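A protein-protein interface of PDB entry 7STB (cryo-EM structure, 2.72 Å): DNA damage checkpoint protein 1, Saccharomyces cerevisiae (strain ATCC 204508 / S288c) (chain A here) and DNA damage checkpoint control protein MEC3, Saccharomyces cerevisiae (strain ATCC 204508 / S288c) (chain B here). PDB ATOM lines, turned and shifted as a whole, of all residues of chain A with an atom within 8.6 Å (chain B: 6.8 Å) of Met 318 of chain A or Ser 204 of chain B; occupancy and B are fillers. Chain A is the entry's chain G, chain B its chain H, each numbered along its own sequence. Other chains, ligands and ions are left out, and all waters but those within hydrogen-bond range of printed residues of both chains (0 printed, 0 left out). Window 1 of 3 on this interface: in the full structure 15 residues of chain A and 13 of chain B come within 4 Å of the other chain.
The backbone NH (N) of Ser 319 of chain A sits at hydrogen-bond distance from the backbone carbonyl oxygen (O) of Ser 204 of chain B. OD1 of Asn 320 of chain A sits close to O of Met 202 of chain B. N of Met 202 of chain B is in hydrogen-bond range of O of Thr 321 of chain A (3.0 Å). The guanidinium group (NH1) of Arg 106 of chain B sits close to the side-chain amide oxygen (OD1) of Asn 277 of chain A, at 2.3 Å.
The backbone carbonyl oxygen (O) of Asn 273 of chain A lies close to the side-chain amide oxygen (OD1) of Asn 277 of chain A (2.9 Å). OG of Ser 296 of chain A lies within hydrogen-bond range of OG1 of Thr 321 of chain A (3.5 Å). The backbone NH of Asn 320 of chain A lies within hydrogen-bond range of the backbone carbonyl oxygen of Ile 297 of chain A (2.9 Å). OG1 of Thr 298 of chain A is in hydrogen-bond range of OG of Ser 317 of chain A, at 3.2 Å. The backbone carbonyl oxygen (O) of Met 318 of chain A lies within hydrogen-bond range of the backbone NH (N) of Ala 299 of chain A, 2.9 Å away. N of His 203 of chain B sits at hydrogen-bond distance from O of Phe 160 of chain B, 2.9 Å away.
Among the printed residues, merely in contact across the chains: Asn 320 of chain A with His 203 of chain B (3.2 Å), Ser 317 of chain A with Lys 206 of chain B (3.5 Å), Leu 316 of chain A with Ser 99 of chain B (3.6 Å), Met 318 of chain A with Phe 205 of chain B (3.7 Å), Leu 316 of chain A with Lys 206 of chain B (3.8 Å), Asn 273 of chain A with Arg 106 of chain B (3.8 Å), Ser 319 of chain A with Met 202 of chain B (3.9 Å), Ser 319 of chain A with His 203 of chain B (3.9 Å), Ser 317 of chain A with Phe 205 of chain B (3.9 Å) and Met 318 of chain A with Ser 204 of chain B (3.9 Å).
Of the printed residues of chain B, Asn 277 of chain A touches Arg 106. Phe 300 of chain A touches none of the printed residues of chain B. Printed residues of chain B within 4 Å of Ser 317 of chain A: Phe 205 and Lys 206. Met 318 of chain A touches just these residues of chain B: Ser 204 and Phe 205. Of the printed residues of chain B, Asn 320 of chain A touches Met 202 and His 203. Of the printed residues of chain A, His 203 of chain B touches Ser 319 and Asn 320. The nearest residue of chain B that does not touch Met 318 of chain A is Ser 102 of chain B (4.8 Å). The nearest residue of chain A that does not touch Ser 204 of chain B is Asn 320 of chain A (4.5 Å). The nearest printed residue of chain B that does not touch Asn 273 of chain A is His 203 of chain B (7.0 Å).
Printed residues of chain B that touch a printed residue of chain A: Ser 99, Arg 106, Met 202, His 203, Ser 204, Phe 205 and Lys 206. Hydrophobic or aromatic side chains of chain B that line the printed part of chain A: Met 202, His 203 and Phe 205. Among the printed residues, 14 pairs touch across the chains. Among the printed residues, no Asp or Glu carboxylate lies within 4 Å of a Lys or Arg side-chain nitrogen of the other chain.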
ATOM      1  N   ASN A 273     -25.676 -35.273   2.063  1.00  0.00           N
ATOM      2  CA  ASN A 273     -25.309 -34.228   1.114  1.00  0.00           C
ATOM      3  C   ASN A 273     -25.146 -32.888   1.815  1.00  0.00           C
ATOM      4  O   ASN A 273     -24.206 -32.138   1.526  1.00  0.00           O
ATOM      5  CB  ASN A 273     -26.362 -34.130   0.010  1.00  0.00           C
ATOM      6  CG  ASN A 273     -26.298 -35.292  -0.960  1.00  0.00           C
ATOM      7  OD1 ASN A 273     -25.239 -35.881  -1.173  1.00  0.00           O
ATOM      8  ND2 ASN A 273     -27.437 -35.628  -1.556  1.00  0.00           N
ATOM      9  N   PHE A 274     -26.054 -32.565   2.740  1.00  0.00           N
ATOM     10  CA  PHE A 274     -25.925 -31.311   3.477  1.00  0.00           C
ATOM     11  C   PHE A 274     -24.656 -31.293   4.321  1.00  0.00           C
ATOM     12  O   PHE A 274     -23.938 -30.287   4.355  1.00  0.00           O
ATOM     13  CB  PHE A 274     -27.148 -31.089   4.366  1.00  0.00           C
ATOM     14  CG  PHE A 274     -26.965 -29.993   5.377  1.00  0.00           C
ATOM     15  CD1 PHE A 274     -26.597 -28.719   4.979  1.00  0.00           C
ATOM     16  CD2 PHE A 274     -27.144 -30.240   6.727  1.00  0.00           C
ATOM     17  CE1 PHE A 274     -26.424 -27.710   5.905  1.00  0.00           C
ATOM     18  CE2 PHE A 274     -26.969 -29.234   7.657  1.00  0.00           C
ATOM     19  CZ  PHE A 274     -26.609 -27.967   7.246  1.00  0.00           C
ATOM     20  N   LEU A 275     -24.359 -32.403   5.002  1.00  0.00           N
ATOM     21  CA  LEU A 275     -23.251 -32.424   5.952  1.00  0.00           C
ATOM     22  C   LEU A 275     -21.901 -32.450   5.251  1.00  0.00           C
ATOM     23  O   LEU A 275     -20.918 -31.928   5.791  1.00  0.00           O
ATOM     24  CB  LEU A 275     -23.389 -33.632   6.879  1.00  0.00           C
ATOM     25  CG  LEU A 275     -24.565 -33.591   7.859  1.00  0.00           C
ATOM     26  CD1 LEU A 275     -24.736 -34.932   8.552  1.00  0.00           C
ATOM     27  CD2 LEU A 275     -24.372 -32.488   8.880  1.00  0.00           C
ATOM     28  N   ASP A 276     -21.823 -33.047   4.060  1.00  0.00           N
ATOM     29  CA  ASP A 276     -20.551 -33.089   3.348  1.00  0.00           C
ATOM     30  C   ASP A 276     -20.031 -31.683   3.075  1.00  0.00           C
ATOM     31  O   ASP A 276     -18.826 -31.427   3.182  1.00  0.00           O
ATOM     32  CB  ASP A 276     -20.707 -33.863   2.039  1.00  0.00           C
ATOM     33  CG  ASP A 276     -20.946 -35.343   2.263  1.00  0.00           C
ATOM     34  OD1 ASP A 276     -20.468 -35.877   3.285  1.00  0.00           O
ATOM     35  OD2 ASP A 276     -21.611 -35.974   1.415  1.00  0.00           O
ATOM     36  N   ASN A 277     -20.926 -30.758   2.725  1.00  0.00           N
ATOM     37  CA  ASN A 277     -20.506 -29.389   2.447  1.00  0.00           C
ATOM     38  C   ASN A 277     -20.136 -28.641   3.721  1.00  0.00           C
ATOM     39  O   ASN A 277     -19.301 -27.731   3.681  1.00  0.00           O
ATOM     40  CB  ASN A 277     -21.616 -28.648   1.702  1.00  0.00           C
ATOM     41  CG  ASN A 277     -21.950 -29.290   0.370  1.00  0.00           C
ATOM     42  OD1 ASN A 277     -23.031 -29.851   0.192  1.00  0.00           O
ATOM     43  ND2 ASN A 277     -21.020 -29.211  -0.574  1.00  0.00           N
ATOM     44  N   CYS A 278     -20.740 -29.003   4.851  1.00  0.00           N
ATOM     45  CA  CYS A 278     -20.467 -28.305   6.100  1.00  0.00           C
ATOM     46  C   CYS A 278     -19.006 -28.464   6.499  1.00  0.00           C
ATOM     47  O   CYS A 278     -18.401 -29.522   6.303  1.00  0.00           O
ATOM     48  CB  CYS A 278     -21.374 -28.835   7.211  1.00  0.00           C
ATOM     49  SG  CYS A 278     -23.092 -28.287   7.101  1.00  0.00           S
ATOM     50  N   ASN A 279     -18.440 -27.401   7.062  1.00  0.00           N
ATOM     51  CA  ASN A 279     -17.074 -27.398   7.569  1.00  0.00           C
ATOM     52  C   ASN A 279     -17.122 -27.240   9.083  1.00  0.00           C
ATOM     53  O   ASN A 279     -17.649 -26.243   9.590  1.00  0.00           O
ATOM     54  CB  ASN A 279     -16.257 -26.275   6.930  1.00  0.00           C
ATOM     55  CG  ASN A 279     -14.860 -26.171   7.503  1.00  0.00           C
ATOM     56  OD1 ASN A 279     -14.328 -27.134   8.054  1.00  0.00           O
ATOM     57  ND2 ASN A 279     -14.253 -24.998   7.371  1.00  0.00           N
ATOM     58  N   VAL A 282     -15.884 -24.057  10.940  1.00  0.00           N
ATOM     59  CA  VAL A 282     -16.695 -22.840  10.906  1.00  0.00           C
ATOM     60  C   VAL A 282     -18.019 -23.036  11.643  1.00  0.00           C
ATOM     61  O   VAL A 282     -18.297 -22.351  12.628  1.00  0.00           O
ATOM     62  CB  VAL A 282     -16.929 -22.370   9.453  1.00  0.00           C
ATOM     63  CG1 VAL A 282     -17.819 -21.138   9.428  1.00  0.00           C
ATOM     64  CG2 VAL A 282     -15.601 -22.084   8.769  1.00  0.00           C
ATOM     65  N   THR A 283     -18.847 -23.971  11.180  1.00  0.00           N
ATOM     66  CA  THR A 283     -20.160 -24.216  11.778  1.00  0.00           C
ATOM     67  C   THR A 283     -20.013 -25.328  12.808  1.00  0.00           C
ATOM     68  O   THR A 283     -20.098 -26.515  12.493  1.00  0.00           O
ATOM     69  CB  THR A 283     -21.187 -24.572  10.711  1.00  0.00           C
ATOM     70  OG1 THR A 283     -20.766 -25.749  10.009  1.00  0.00           O
ATOM     71  CG2 THR A 283     -21.354 -23.425   9.726  1.00  0.00           C
ATOM     72  N   GLU A 285     -21.938 -25.858  15.665  1.00  0.00           N
ATOM     73  CA  GLU A 285     -23.178 -26.394  16.207  1.00  0.00           C
ATOM     74  C   GLU A 285     -24.115 -26.819  15.085  1.00  0.00           C
ATOM     75  O   GLU A 285     -24.049 -26.301  13.969  1.00  0.00           O
ATOM     76  CB  GLU A 285     -23.870 -25.361  17.098  1.00  0.00           C
ATOM     77  CG  GLU A 285     -23.051 -24.938  18.305  1.00  0.00           C
ATOM     78  CD  GLU A 285     -22.796 -26.079  19.268  1.00  0.00           C
ATOM     79  OE1 GLU A 285     -23.777 -26.644  19.795  1.00  0.00           O
ATOM     80  OE2 GLU A 285     -21.613 -26.413  19.500  1.00  0.00           O
ATOM     81  N   VAL A 286     -24.992 -27.773  15.392  1.00  0.00           N
ATOM     82  CA  VAL A 286     -26.031 -28.220  14.473  1.00  0.00           C
ATOM     83  C   VAL A 286     -27.361 -28.183  15.211  1.00  0.00           C
ATOM     84  O   VAL A 286     -27.475 -28.701  16.329  1.00  0.00           O
ATOM     85  CB  VAL A 286     -25.747 -29.631  13.925  1.00  0.00           C
ATOM     86  CG1 VAL A 286     -25.788 -30.662  15.039  1.00  0.00           C
ATOM     87  CG2 VAL A 286     -26.743 -29.985  12.832  1.00  0.00           C
ATOM     88  N   LYS A 287     -28.364 -27.571  14.584  1.00  0.00           N
ATOM     89  CA  LYS A 287     -29.681 -27.392  15.176  1.00  0.00           C
ATOM     90  C   LYS A 287     -30.738 -27.983  14.255  1.00  0.00           C
ATOM     91  O   LYS A 287     -30.743 -27.716  13.047  1.00  0.00           O
ATOM     92  CB  LYS A 287     -29.964 -25.910  15.430  1.00  0.00           C
ATOM     93  CG  LYS A 287     -31.352 -25.619  15.977  1.00  0.00           C
ATOM     94  CD  LYS A 287     -31.443 -24.230  16.608  1.00  0.00           C
ATOM     95  CE  LYS A 287     -30.700 -23.173  15.800  1.00  0.00           C
ATOM     96  NZ  LYS A 287     -30.959 -21.798  16.310  1.00  0.00           N
ATOM     97  N   SER A 296     -36.152 -28.567   9.345  1.00  0.00           N
ATOM     98  CA  SER A 296     -35.016 -27.725   8.998  1.00  0.00           C
ATOM     99  C   SER A 296     -33.791 -28.188   9.773  1.00  0.00           C
ATOM    100  O   SER A 296     -33.878 -28.462  10.975  1.00  0.00           O
ATOM    101  CB  SER A 296     -35.311 -26.254   9.303  1.00  0.00           C
ATOM    102  OG  SER A 296     -34.155 -25.456   9.124  1.00  0.00           O
ATOM    103  N   ILE A 297     -32.659 -28.284   9.082  1.00  0.00           N
ATOM    104  CA  ILE A 297     -31.380 -28.620   9.698  1.00  0.00           C
ATOM    105  C   ILE A 297     -30.410 -27.500   9.359  1.00  0.00           C
ATOM    106  O   ILE A 297     -30.199 -27.195   8.179  1.00  0.00           O
ATOM    107  CB  ILE A 297     -30.847 -29.979   9.216  1.00  0.00           C
ATOM    108  CG1 ILE A 297     -29.531 -30.311   9.921  1.00  0.00           C
ATOM    109  CG2 ILE A 297     -30.647 -29.982   7.706  1.00  0.00           C
ATOM    110  CD1 ILE A 297     -29.047 -31.721   9.678  1.00  0.00           C
ATOM    111  N   THR A 298     -29.827 -26.883  10.385  1.00  0.00           N
ATOM    112  CA  THR A 298     -28.952 -25.733  10.191  1.00  0.00           C
ATOM    113  C   THR A 298     -27.647 -25.947  10.939  1.00  0.00           C
ATOM    114  O   THR A 298     -27.652 -26.186  12.151  1.00  0.00           O
ATOM    115  CB  THR A 298     -29.633 -24.437  10.649  1.00  0.00           C
ATOM    116  OG1 THR A 298     -28.741 -23.331  10.461  1.00  0.00           O
ATOM    117  CG2 THR A 298     -30.031 -24.514  12.112  1.00  0.00           C
ATOM    118  N   ALA A 299     -26.535 -25.866  10.217  1.00  0.00           N
ATOM    119  CA  ALA A 299     -25.213 -25.805  10.820  1.00  0.00           C
ATOM    120  C   ALA A 299     -24.888 -24.342  11.088  1.00  0.00           C
ATOM    121  O   ALA A 299     -24.853 -23.529  10.158  1.00  0.00           O
ATOM    122  CB  ALA A 299     -24.167 -26.443   9.908  1.00  0.00           C
ATOM    123  N   PHE A 300     -24.661 -24.007  12.355  1.00  0.00           N
ATOM    124  CA  PHE A 300     -24.585 -22.618  12.777  1.00  0.00           C
ATOM    125  C   PHE A 300     -23.496 -22.441  13.826  1.00  0.00           C
ATOM    126  O   PHE A 300     -22.958 -23.404  14.384  1.00  0.00           O
ATOM    127  CB  PHE A 300     -25.933 -22.135  13.328  1.00  0.00           C
ATOM    128  CG  PHE A 300     -26.195 -22.560  14.742  1.00  0.00           C
ATOM    129  CD1 PHE A 300     -26.677 -23.828  15.020  1.00  0.00           C
ATOM    130  CD2 PHE A 300     -25.960 -21.694  15.795  1.00  0.00           C
ATOM    131  CE1 PHE A 300     -26.918 -24.222  16.319  1.00  0.00           C
ATOM    132  CE2 PHE A 300     -26.199 -22.085  17.097  1.00  0.00           C
ATOM    133  CZ  PHE A 300     -26.679 -23.350  17.358  1.00  0.00           C
ATOM    134  N   THR A 301     -23.185 -21.171  14.078  1.00  0.00           N
ATOM    135  CA  THR A 301     -22.225 -20.749  15.085  1.00  0.00           C
ATOM    136  C   THR A 301     -22.789 -19.538  15.814  1.00  0.00           C
ATOM    137  O   THR A 301     -23.551 -18.753  15.243  1.00  0.00           O
ATOM    138  CB  THR A 301     -20.869 -20.395  14.452  1.00  0.00           C
ATOM    139  OG1 THR A 301     -20.340 -21.542  13.775  1.00  0.00           O
ATOM    140  CG2 THR A 301     -19.877 -19.929  15.507  1.00  0.00           C
ATOM    141  N   ALA A 315     -20.188 -15.260  13.221  1.00  0.00           N
ATOM    142  CA  ALA A 315     -21.303 -16.195  13.171  1.00  0.00           C
ATOM    143  C   ALA A 315     -21.709 -16.442  11.724  1.00  0.00           C
ATOM    144  O   ALA A 315     -21.907 -15.493  10.959  1.00  0.00           O
ATOM    145  CB  ALA A 315     -22.494 -15.661  13.966  1.00  0.00           C
ATOM    146  N   LEU A 316     -21.835 -17.715  11.359  1.00  0.00           N
ATOM    147  CA  LEU A 316     -22.278 -18.117  10.033  1.00  0.00           C
ATOM    148  C   LEU A 316     -23.345 -19.191  10.176  1.00  0.00           C
ATOM    149  O   LEU A 316     -23.322 -19.988  11.117  1.00  0.00           O
ATOM    150  CB  LEU A 316     -21.106 -18.637   9.182  1.00  0.00           C
ATOM    151  CG  LEU A 316     -21.446 -19.297   7.841  1.00  0.00           C
ATOM    152  CD1 LEU A 316     -21.825 -18.249   6.808  1.00  0.00           C
ATOM    153  CD2 LEU A 316     -20.279 -20.134   7.349  1.00  0.00           C
ATOM    154  N   SER A 317     -24.285 -19.203   9.234  1.00  0.00           N
ATOM    155  CA  SER A 317     -25.384 -20.156   9.241  1.00  0.00           C
ATOM    156  C   SER A 317     -25.513 -20.807   7.872  1.00  0.00           C
ATOM    157  O   SER A 317     -25.247 -20.184   6.841  1.00  0.00           O
ATOM    158  CB  SER A 317     -26.708 -19.482   9.624  1.00  0.00           C
ATOM    159  OG  SER A 317     -27.783 -20.400   9.561  1.00  0.00           O
ATOM    160  N   MET A 318     -25.925 -22.072   7.878  1.00  0.00           N
ATOM    161  CA  MET A 318     -26.116 -22.834   6.646  1.00  0.00           C
ATOM    162  C   MET A 318     -27.261 -23.805   6.893  1.00  0.00           C
ATOM    163  O   MET A 318     -27.080 -24.802   7.595  1.00  0.00           O
ATOM    164  CB  MET A 318     -24.838 -23.574   6.260  1.00  0.00           C
ATOM    165  CG  MET A 318     -24.907 -24.298   4.931  1.00  0.00           C
ATOM    166  SD  MET A 318     -23.366 -25.144   4.525  1.00  0.00           S
ATOM    167  CE  MET A 318     -22.304 -23.753   4.141  1.00  0.00           C
ATOM    168  N   SER A 319     -28.430 -23.518   6.327  1.00  0.00           N
ATOM    169  CA  SER A 319     -29.646 -24.252   6.642  1.00  0.00           C
ATOM    170  C   SER A 319     -30.235 -24.894   5.393  1.00  0.00           C
ATOM    171  O   SER A 319     -30.140 -24.352   4.288  1.00  0.00           O
ATOM    172  CB  SER A 319     -30.691 -23.332   7.284  1.00  0.00           C
ATOM    173  OG  SER A 319     -30.774 -22.096   6.596  1.00  0.00           O
ATOM    174  N   ASN A 320     -30.841 -26.065   5.586  1.00  0.00           N
ATOM    175  CA  ASN A 320     -31.620 -26.739   4.558  1.00  0.00           C
ATOM    176  C   ASN A 320     -32.961 -27.148   5.149  1.00  0.00           C
ATOM    177  O   ASN A 320     -33.012 -27.729   6.238  1.00  0.00           O
ATOM    178  CB  ASN A 320     -30.893 -27.968   4.004  1.00  0.00           C
ATOM    179  CG  ASN A 320     -29.867 -27.611   2.948  1.00  0.00           C
ATOM    180  OD1 ASN A 320     -30.059 -26.678   2.171  1.00  0.00           O
ATOM    181  ND2 ASN A 320     -28.779 -28.367   2.901  1.00  0.00           N
ATOM    182  N   THR A 321     -34.036 -26.851   4.425  1.00  0.00           N
ATOM    183  CA  THR A 321     -35.394 -27.125   4.871  1.00  0.00           C
ATOM    184  C   THR A 321     -36.101 -28.008   3.853  1.00  0.00           C
ATOM    185  O   THR A 321     -35.958 -27.811   2.642  1.00  0.00           O
ATOM    186  CB  THR A 321     -36.184 -25.826   5.067  1.00  0.00           C
ATOM    187  OG1 THR A 321     -35.473 -24.961   5.960  1.00  0.00           O
ATOM    188  CG2 THR A 321     -37.564 -26.115   5.637  1.00  0.00           C
ATOM    189  N   LEU A 360     -21.747 -30.981  15.686  1.00  0.00           N
ATOM    190  CA  LEU A 360     -21.840 -31.344  14.277  1.00  0.00           C
ATOM    191  C   LEU A 360     -20.785 -32.353  13.840  1.00  0.00           C
ATOM    192  O   LEU A 360     -21.078 -33.222  13.014  1.00  0.00           O
ATOM    193  CB  LEU A 360     -21.722 -30.084  13.413  1.00  0.00           C
ATOM    194  CG  LEU A 360     -21.686 -30.261  11.893  1.00  0.00           C
ATOM    195  CD1 LEU A 360     -23.034 -30.717  11.371  1.00  0.00           C
ATOM    196  CD2 LEU A 360     -21.262 -28.969  11.223  1.00  0.00           C
ATOM    197  N   SER B  99     -17.258 -17.667   2.681  1.00  0.00           N
ATOM    198  CA  SER B  99     -18.677 -17.996   2.798  1.00  0.00           C
ATOM    199  C   SER B  99     -19.378 -17.893   1.448  1.00  0.00           C
ATOM    200  O   SER B  99     -20.101 -18.811   1.035  1.00  0.00           O
ATOM    201  CB  SER B  99     -19.341 -17.074   3.821  1.00  0.00           C
ATOM    202  OG  SER B  99     -18.762 -17.236   5.104  1.00  0.00           O
ATOM    203  N   SER B 102     -18.259 -20.753  -0.777  1.00  0.00           N
ATOM    204  CA  SER B 102     -18.916 -22.017  -0.460  1.00  0.00           C
ATOM    205  C   SER B 102     -20.346 -22.036  -0.981  1.00  0.00           C
ATOM    206  O   SER B 102     -20.800 -23.041  -1.545  1.00  0.00           O
ATOM    207  CB  SER B 102     -18.893 -22.249   1.050  1.00  0.00           C
ATOM    208  OG  SER B 102     -17.564 -22.288   1.539  1.00  0.00           O
ATOM    209  N   VAL B 103     -21.074 -20.932  -0.800  1.00  0.00           N
ATOM    210  CA  VAL B 103     -22.435 -20.861  -1.323  1.00  0.00           C
ATOM    211  C   VAL B 103     -22.423 -21.019  -2.837  1.00  0.00           C
ATOM    212  O   VAL B 103     -23.309 -21.656  -3.422  1.00  0.00           O
ATOM    213  CB  VAL B 103     -23.105 -19.542  -0.895  1.00  0.00           C
ATOM    214  CG1 VAL B 103     -24.462 -19.392  -1.569  1.00  0.00           C
ATOM    215  CG2 VAL B 103     -23.250 -19.488   0.615  1.00  0.00           C
ATOM    216  N   ARG B 106     -21.937 -24.600  -3.774  1.00  0.00           N
ATOM    217  CA  ARG B 106     -23.197 -25.309  -3.572  1.00  0.00           C
ATOM    218  C   ARG B 106     -24.146 -25.061  -4.739  1.00  0.00           C
ATOM    219  O   ARG B 106     -24.739 -25.997  -5.289  1.00  0.00           O
ATOM    220  CB  ARG B 106     -23.823 -24.864  -2.249  1.00  0.00           C
ATOM    221  CG  ARG B 106     -25.181 -25.475  -1.881  1.00  0.00           C
ATOM    222  CD  ARG B 106     -25.136 -26.954  -1.500  1.00  0.00           C
ATOM    223  NE  ARG B 106     -25.216 -27.865  -2.635  1.00  0.00           N
ATOM    224  CZ  ARG B 106     -25.041 -29.177  -2.549  1.00  0.00           C
ATOM    225  NH1 ARG B 106     -24.724 -29.759  -1.403  1.00  0.00           N
ATOM    226  NH2 ARG B 106     -25.199 -29.927  -3.635  1.00  0.00           N
ATOM    227  N   GLY B 157     -28.950 -13.035   2.782  1.00  0.00           N
ATOM    228  CA  GLY B 157     -29.828 -14.189   2.781  1.00  0.00           C
ATOM    229  C   GLY B 157     -29.892 -14.888   1.440  1.00  0.00           C
ATOM    230  O   GLY B 157     -30.905 -14.801   0.738  1.00  0.00           O
ATOM    231  N   ILE B 158     -28.824 -15.584   1.069  1.00  0.00           N
ATOM    232  CA  ILE B 158     -28.759 -16.239  -0.233  1.00  0.00           C
ATOM    233  C   ILE B 158     -29.614 -17.499  -0.183  1.00  0.00           C
ATOM    234  O   ILE B 158     -29.357 -18.403   0.616  1.00  0.00           O
ATOM    235  CB  ILE B 158     -27.310 -16.567  -0.620  1.00  0.00           C
ATOM    236  CG1 ILE B 158     -26.406 -15.355  -0.365  1.00  0.00           C
ATOM    237  CG2 ILE B 158     -27.239 -16.993  -2.080  1.00  0.00           C
ATOM    238  CD1 ILE B 158     -24.973 -15.548  -0.810  1.00  0.00           C
ATOM    239  N   THR B 159     -30.635 -17.561  -1.037  1.00  0.00           N
ATOM    240  CA  THR B 159     -31.586 -18.664  -1.035  1.00  0.00           C
ATOM    241  C   THR B 159     -31.773 -19.190  -2.448  1.00  0.00           C
ATOM    242  O   THR B 159     -31.971 -18.410  -3.385  1.00  0.00           O
ATOM    243  CB  THR B 159     -32.937 -18.226  -0.459  1.00  0.00           C
ATOM    244  OG1 THR B 159     -33.400 -17.057  -1.149  1.00  0.00           O
ATOM    245  CG2 THR B 159     -32.815 -17.922   1.025  1.00  0.00           C
ATOM    246  N   PHE B 160     -31.714 -20.513  -2.597  1.00  0.00           N
ATOM    247  CA  PHE B 160     -32.033 -21.155  -3.865  1.00  0.00           C
ATOM    248  C   PHE B 160     -32.551 -22.557  -3.593  1.00  0.00           C
ATOM    249  O   PHE B 160     -32.306 -23.135  -2.534  1.00  0.00           O
ATOM    250  CB  PHE B 160     -30.823 -21.204  -4.809  1.00  0.00           C
ATOM    251  CG  PHE B 160     -29.596 -21.821  -4.205  1.00  0.00           C
ATOM    252  CD1 PHE B 160     -29.423 -23.195  -4.201  1.00  0.00           C
ATOM    253  CD2 PHE B 160     -28.603 -21.026  -3.660  1.00  0.00           C
ATOM    254  CE1 PHE B 160     -28.291 -23.763  -3.654  1.00  0.00           C
ATOM    255  CE2 PHE B 160     -27.468 -21.588  -3.112  1.00  0.00           C
ATOM    256  CZ  PHE B 160     -27.312 -22.959  -3.108  1.00  0.00           C
ATOM    257  N   MET B 202     -34.959 -26.626   0.113  1.00  0.00           N
ATOM    258  CA  MET B 202     -34.664 -25.204   0.211  1.00  0.00           C
ATOM    259  C   MET B 202     -33.282 -25.006   0.817  1.00  0.00           C
ATOM    260  O   MET B 202     -33.013 -25.458   1.933  1.00  0.00           O
ATOM    261  CB  MET B 202     -35.719 -24.496   1.059  1.00  0.00           C
ATOM    262  CG  MET B 202     -37.020 -24.215   0.329  1.00  0.00           C
ATOM    263  SD  MET B 202     -38.083 -25.666   0.217  1.00  0.00           S
ATOM    264  CE  MET B 202     -38.734 -25.739   1.885  1.00  0.00           C
ATOM    265  N   HIS B 203     -32.409 -24.327   0.080  1.00  0.00           N
ATOM    266  CA  HIS B 203     -31.063 -24.002   0.533  1.00  0.00           C
ATOM    267  C   HIS B 203     -31.026 -22.527   0.906  1.00  0.00           C
ATOM    268  O   HIS B 203     -31.307 -21.665   0.064  1.00  0.00           O
ATOM    269  CB  HIS B 203     -30.027 -24.306  -0.550  1.00  0.00           C
ATOM    270  CG  HIS B 203     -29.875 -25.764  -0.850  1.00  0.00           C
ATOM    271  ND1 HIS B 203     -30.925 -26.551  -1.274  1.00  0.00           N
ATOM    272  CD2 HIS B 203     -28.794 -26.578  -0.795  1.00  0.00           C
ATOM    273  CE1 HIS B 203     -30.499 -27.787  -1.462  1.00  0.00           C
ATOM    274  NE2 HIS B 203     -29.209 -27.830  -1.178  1.00  0.00           N
ATOM    275  N   SER B 204     -30.682 -22.245   2.161  1.00  0.00           N
ATOM    276  CA  SER B 204     -30.615 -20.887   2.680  1.00  0.00           C
ATOM    277  C   SER B 204     -29.280 -20.679   3.379  1.00  0.00           C
ATOM    278  O   SER B 204     -28.780 -21.578   4.060  1.00  0.00           O
ATOM    279  CB  SER B 204     -31.766 -20.610   3.654  1.00  0.00           C
ATOM    280  OG  SER B 204     -31.682 -19.298   4.182  1.00  0.00           O
ATOM    281  N   PHE B 205     -28.707 -19.491   3.202  1.00  0.00           N
ATOM    282  CA  PHE B 205     -27.408 -19.156   3.774  1.00  0.00           C
ATOM    283  C   PHE B 205     -27.449 -17.719   4.264  1.00  0.00           C
ATOM    284  O   PHE B 205     -27.705 -16.802   3.477  1.00  0.00           O
ATOM    285  CB  PHE B 205     -26.285 -19.335   2.747  1.00  0.00           C
ATOM    286  CG  PHE B 205     -26.366 -20.620   1.976  1.00  0.00           C
ATOM    287  CD1 PHE B 205     -27.205 -20.736   0.882  1.00  0.00           C
ATOM    288  CD2 PHE B 205     -25.600 -21.713   2.343  1.00  0.00           C
ATOM    289  CE1 PHE B 205     -27.283 -21.915   0.174  1.00  0.00           C
ATOM    290  CE2 PHE B 205     -25.674 -22.895   1.634  1.00  0.00           C
ATOM    291  CZ  PHE B 205     -26.517 -22.994   0.549  1.00  0.00           C
ATOM    292  N   LYS B 206     -27.197 -17.525   5.558  1.00  0.00           N
ATOM    293  CA  LYS B 206     -27.099 -16.194   6.157  1.00  0.00           C
ATOM    294  C   LYS B 206     -25.615 -15.880   6.299  1.00  0.00           C
ATOM    295  O   LYS B 206     -24.980 -16.219   7.298  1.00  0.00           O
ATOM    296  CB  LYS B 206     -27.819 -16.140   7.500  1.00  0.00           C
ATOM    297  CG  LYS B 206     -29.291 -16.508   7.439  1.00  0.00           C
ATOM    298  CD  LYS B 206     -30.118 -15.410   6.793  1.00  0.00           C
ATOM    299  CE  LYS B 206     -31.602 -15.736   6.838  1.00  0.00           C
ATOM    300  NZ  LYS B 206     -32.429 -14.686   6.181  1.00  0.00           N
